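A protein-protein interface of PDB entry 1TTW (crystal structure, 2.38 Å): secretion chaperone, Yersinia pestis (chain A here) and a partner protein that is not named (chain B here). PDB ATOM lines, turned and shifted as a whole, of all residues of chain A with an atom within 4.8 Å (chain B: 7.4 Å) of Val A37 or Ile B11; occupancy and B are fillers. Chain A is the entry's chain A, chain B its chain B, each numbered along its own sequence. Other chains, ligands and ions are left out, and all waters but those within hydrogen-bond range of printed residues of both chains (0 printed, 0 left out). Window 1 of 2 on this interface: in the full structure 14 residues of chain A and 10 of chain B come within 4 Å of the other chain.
The side-chain hydroxyl (OG1) of Thr A31 is in hydrogen-bond range of the backbone carbonyl oxygen (O) of Ile B11, at 3.0 Å.
N of Gln B9 is in hydrogen-bond range of O of Thr A31 (3.0 Å).
The backbone carbonyl oxygen of His A39 lies within hydrogen-bond range of the backbone NH of Phe A51.
Among the printed residues, pairs that only touch across the chains: Ala A29 with Ile B11 (3.95 Å), Val A37 with Ile B11 (3.95 Å), His A39 with Glu B15 (3.8 Å) and Arg A53 with Phe B18 (3.8 Å).
Of chain B, only Ile B11 (3.95 Å) comes within 4 Å of Val A37.
Of chain A, only Ala A29, Thr A31 and Val A37 come within 4 Å of Ile B11.
Of the printed residues of chain B, Arg A53 touches Phe B18.
Printed residues of chain A within 4 Å of Glu B15: His A39.
Ser B13 touches none of the printed residues of chain A.
The nearest residue of chain B that does not touch Val A37 is Thr B12 (4.6 Å).
The nearest printed residue of chain B that does not touch Arg A53 is Glu B15 (7.5 Å).
Hydrophobic or aromatic side chains of chain A within 4 Å of the printed part of chain B: Ala A29, Val A37 and His A39.
Along chain A the printed residues that touch a printed residue of chain B span positions 29 to 53.
Among the printed residues, no Asp or Glu carboxylate lies within 4 Å of a Lys or Arg side-chain nitrogen of the other chain.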
ATOM      1  N   ALA A  29      15.393  12.090  23.332  1.00  0.00           N
ATOM      2  CA  ALA A  29      14.303  12.676  22.610  1.00  0.00           C
ATOM      3  C   ALA A  29      13.019  12.479  23.425  1.00  0.00           C
ATOM      4  O   ALA A  29      12.875  11.517  24.210  1.00  0.00           O
ATOM      5  CB  ALA A  29      14.212  12.045  21.315  1.00  0.00           C
ATOM      6  N   VAL A  30      12.048  13.348  23.198  1.00  0.00           N
ATOM      7  CA  VAL A  30      10.740  13.212  23.878  1.00  0.00           C
ATOM      8  C   VAL A  30       9.761  13.474  22.785  1.00  0.00           C
ATOM      9  O   VAL A  30      10.069  14.248  21.830  1.00  0.00           O
ATOM     10  CB  VAL A  30      10.663  14.194  25.008  1.00  0.00           C
ATOM     11  CG1 VAL A  30       9.305  14.616  25.227  1.00  0.00           C
ATOM     12  CG2 VAL A  30      11.151  13.599  26.270  1.00  0.00           C
ATOM     13  N   THR A  31       8.585  12.795  22.810  1.00  0.00           N
ATOM     14  CA  THR A  31       7.475  13.188  21.856  1.00  0.00           C
ATOM     15  C   THR A  31       6.365  13.901  22.591  1.00  0.00           C
ATOM     16  O   THR A  31       6.077  13.599  23.749  1.00  0.00           O
ATOM     17  CB  THR A  31       6.984  12.054  20.982  1.00  0.00           C
ATOM     18  OG1 THR A  31       8.104  11.262  20.561  1.00  0.00           O
ATOM     19  CG2 THR A  31       6.341  12.582  19.554  1.00  0.00           C
ATOM     20  N   ILE A  35       3.016  14.709  18.058  1.00  0.00           N
ATOM     21  CA  ILE A  35       3.473  15.254  16.746  1.00  0.00           C
ATOM     22  C   ILE A  35       4.945  15.843  16.729  1.00  0.00           C
ATOM     23  O   ILE A  35       5.635  15.899  15.708  1.00  0.00           O
ATOM     24  CB  ILE A  35       2.627  16.506  16.411  1.00  0.00           C
ATOM     25  CG1 ILE A  35       1.231  16.485  16.998  1.00  0.00           C
ATOM     26  CG2 ILE A  35       2.558  16.795  14.912  1.00  0.00           C
ATOM     27  CD1 ILE A  35       0.406  17.759  16.441  1.00  0.00           C
ATOM     28  N   TRP A  36       5.310  16.396  17.885  1.00  0.00           N
ATOM     29  CA  TRP A  36       6.531  17.115  18.100  1.00  0.00           C
ATOM     30  C   TRP A  36       7.559  16.261  18.787  1.00  0.00           C
ATOM     31  O   TRP A  36       7.341  15.689  19.843  1.00  0.00           O
ATOM     32  CB  TRP A  36       6.209  18.193  19.028  1.00  0.00           C
ATOM     33  CG  TRP A  36       5.136  19.103  18.578  1.00  0.00           C
ATOM     34  CD1 TRP A  36       3.986  19.441  19.314  1.00  0.00           C
ATOM     35  CD2 TRP A  36       5.095  19.876  17.405  1.00  0.00           C
ATOM     36  NE1 TRP A  36       3.276  20.398  18.648  1.00  0.00           N
ATOM     37  CE2 TRP A  36       3.874  20.639  17.444  1.00  0.00           C
ATOM     38  CE3 TRP A  36       5.871  19.943  16.278  1.00  0.00           C
ATOM     39  CZ2 TRP A  36       3.488  21.524  16.439  1.00  0.00           C
ATOM     40  CZ3 TRP A  36       5.455  20.812  15.224  1.00  0.00           C
ATOM     41  CH2 TRP A  36       4.275  21.588  15.337  1.00  0.00           C
ATOM     42  N   VAL A  37       8.694  16.146  18.143  1.00  0.00           N
ATOM     43  CA  VAL A  37       9.906  15.525  18.814  1.00  0.00           C
ATOM     44  C   VAL A  37      10.853  16.598  19.235  1.00  0.00           C
ATOM     45  O   VAL A  37      11.270  17.420  18.409  1.00  0.00           O
ATOM     46  CB  VAL A  37      10.697  14.550  17.958  1.00  0.00           C
ATOM     47  CG1 VAL A  37      11.443  13.434  18.876  1.00  0.00           C
ATOM     48  CG2 VAL A  37       9.776  13.944  16.896  1.00  0.00           C
ATOM     49  N   VAL A  38      11.104  16.611  20.538  1.00  0.00           N
ATOM     50  CA  VAL A  38      12.064  17.453  21.171  1.00  0.00           C
ATOM     51  C   VAL A  38      13.301  16.620  21.551  1.00  0.00           C
ATOM     52  O   VAL A  38      13.212  15.708  22.386  1.00  0.00           O
ATOM     53  CB  VAL A  38      11.568  18.089  22.417  1.00  0.00           C
ATOM     54  CG1 VAL A  38      12.713  18.913  23.052  1.00  0.00           C
ATOM     55  CG2 VAL A  38      10.453  19.031  22.046  1.00  0.00           C
ATOM     56  N   HIS A  39      14.415  16.979  20.893  1.00  0.00           N
ATOM     57  CA  HIS A  39      15.799  16.451  21.151  1.00  0.00           C
ATOM     58  C   HIS A  39      16.475  17.187  22.192  1.00  0.00           C
ATOM     59  O   HIS A  39      16.358  18.420  22.229  1.00  0.00           O
ATOM     60  CB  HIS A  39      16.563  16.634  19.890  1.00  0.00           C
ATOM     61  CG  HIS A  39      15.973  15.835  18.787  1.00  0.00           C
ATOM     62  ND1 HIS A  39      15.792  14.487  18.888  1.00  0.00           N
ATOM     63  CD2 HIS A  39      15.471  16.202  17.578  1.00  0.00           C
ATOM     64  CE1 HIS A  39      15.326  14.044  17.723  1.00  0.00           C
ATOM     65  NE2 HIS A  39      15.073  15.065  16.936  1.00  0.00           N
ATOM     66  N   PHE A  51      16.034  20.971  21.336  1.00  0.00           N
ATOM     67  CA  PHE A  51      15.646  21.420  19.997  1.00  0.00           C
ATOM     68  C   PHE A  51      14.702  20.637  19.187  1.00  0.00           C
ATOM     69  O   PHE A  51      14.445  19.459  19.440  1.00  0.00           O
ATOM     70  CB  PHE A  51      16.907  21.607  19.178  1.00  0.00           C
ATOM     71  CG  PHE A  51      17.635  20.364  18.807  1.00  0.00           C
ATOM     72  CD1 PHE A  51      17.445  19.785  17.613  1.00  0.00           C
ATOM     73  CD2 PHE A  51      18.604  19.915  19.590  1.00  0.00           C
ATOM     74  CE1 PHE A  51      18.240  18.648  17.242  1.00  0.00           C
ATOM     75  CE2 PHE A  51      19.378  18.830  19.239  1.00  0.00           C
ATOM     76  CZ  PHE A  51      19.181  18.153  18.080  1.00  0.00           C
ATOM     77  N   MET A  52      14.179  21.243  18.125  1.00  0.00           N
ATOM     78  CA  MET A  52      13.225  20.523  17.302  1.00  0.00           C
ATOM     79  C   MET A  52      12.925  21.021  15.986  1.00  0.00           C
ATOM     80  O   MET A  52      12.973  22.180  15.778  1.00  0.00           O
ATOM     81  CB  MET A  52      11.779  20.563  18.005  1.00  0.00           C
ATOM     82  CG  MET A  52      11.059  21.859  17.947  1.00  0.00           C
ATOM     83  SD  MET A  52       9.314  21.840  19.059  1.00  0.00           S
ATOM     84  CE  MET A  52       8.609  20.637  18.345  1.00  0.00           C
ATOM     85  N   ARG A  53      12.511  20.128  15.115  1.00  0.00           N
ATOM     86  CA  ARG A  53      11.979  20.485  13.787  1.00  0.00           C
ATOM     87  C   ARG A  53      10.489  20.931  13.858  1.00  0.00           C
ATOM     88  O   ARG A  53       9.735  20.391  14.619  1.00  0.00           O
ATOM     89  CB  ARG A  53      12.231  19.249  12.758  1.00  0.00           C
ATOM     90  N   GLN B   9       4.602  12.282  26.013  1.00  0.00           N
ATOM     91  CA  GLN B   9       5.741  11.401  26.490  1.00  0.00           C
ATOM     92  C   GLN B   9       6.681  10.501  25.499  1.00  0.00           C
ATOM     93  O   GLN B   9       6.605  10.624  24.293  1.00  0.00           O
ATOM     94  CB  GLN B   9       5.226  10.560  27.667  1.00  0.00           C
ATOM     95  N   ALA B  10       7.510   9.592  26.083  1.00  0.00           N
ATOM     96  CA  ALA B  10       8.869   9.070  25.637  1.00  0.00           C
ATOM     97  C   ALA B  10       9.221   8.292  24.317  1.00  0.00           C
ATOM     98  O   ALA B  10       9.250   7.104  24.419  1.00  0.00           O
ATOM     99  CB  ALA B  10       9.461   8.153  26.890  1.00  0.00           C
ATOM    100  N   ILE B  11       9.600   8.873  23.155  1.00  0.00           N
ATOM    101  CA  ILE B  11      10.184   8.024  22.019  1.00  0.00           C
ATOM    102  C   ILE B  11      10.827   8.765  20.752  1.00  0.00           C
ATOM    103  O   ILE B  11      10.875  10.005  20.758  1.00  0.00           O
ATOM    104  CB  ILE B  11       9.137   6.863  21.535  1.00  0.00           C
ATOM    105  N   THR B  12      11.282   7.990  19.700  1.00  0.00           N
ATOM    106  CA  THR B  12      11.861   8.481  18.355  1.00  0.00           C
ATOM    107  C   THR B  12      11.966   7.450  17.083  1.00  0.00           C
ATOM    108  O   THR B  12      11.581   6.263  17.193  1.00  0.00           O
ATOM    109  CB  THR B  12      13.261   9.176  18.587  1.00  0.00           C
ATOM    110  N   SER B  13      12.503   7.935  15.917  1.00  0.00           N
ATOM    111  CA  SER B  13      12.500   7.231  14.576  1.00  0.00           C
ATOM    112  C   SER B  13      13.622   7.659  13.503  1.00  0.00           C
ATOM    113  O   SER B  13      14.721   7.097  13.558  1.00  0.00           O
ATOM    114  CB  SER B  13      11.041   7.199  14.005  1.00  0.00           C
ATOM    115  OG  SER B  13      10.869   7.793  12.724  1.00  0.00           O
ATOM    116  N   GLU B  15      15.538  10.544  12.853  1.00  0.00           N
ATOM    117  CA  GLU B  15      15.986  11.747  13.501  1.00  0.00           C
ATOM    118  C   GLU B  15      17.285  11.417  14.354  1.00  0.00           C
ATOM    119  O   GLU B  15      18.269  12.196  14.341  1.00  0.00           O
ATOM    120  CB  GLU B  15      14.798  12.344  14.331  1.00  0.00           C
ATOM    121  N   PHE B  18      17.979  12.997  11.366  1.00  0.00           N
ATOM    122  CA  PHE B  18      17.836  14.497  11.376  1.00  0.00           C
ATOM    123  C   PHE B  18      18.434  15.227  12.609  1.00  0.00           C
ATOM    124  O   PHE B  18      18.938  16.381  12.531  1.00  0.00           O
ATOM    125  CB  PHE B  18      16.368  14.948  11.307  1.00  0.00           C
ATOM    126  CG  PHE B  18      16.189  16.379  11.768  1.00  0.00           C
ATOM    127  CD1 PHE B  18      16.259  17.429  10.844  1.00  0.00           C
ATOM    128  CD2 PHE B  18      16.073  16.681  13.129  1.00  0.00           C
ATOM    129  CE1 PHE B  18      16.142  18.720  11.249  1.00  0.00           C
ATOM    130  CE2 PHE B  18      15.979  17.967  13.543  1.00  0.00           C
ATOM    131  CZ  PHE B  18      16.007  18.995  12.611  1.00  0.00           C
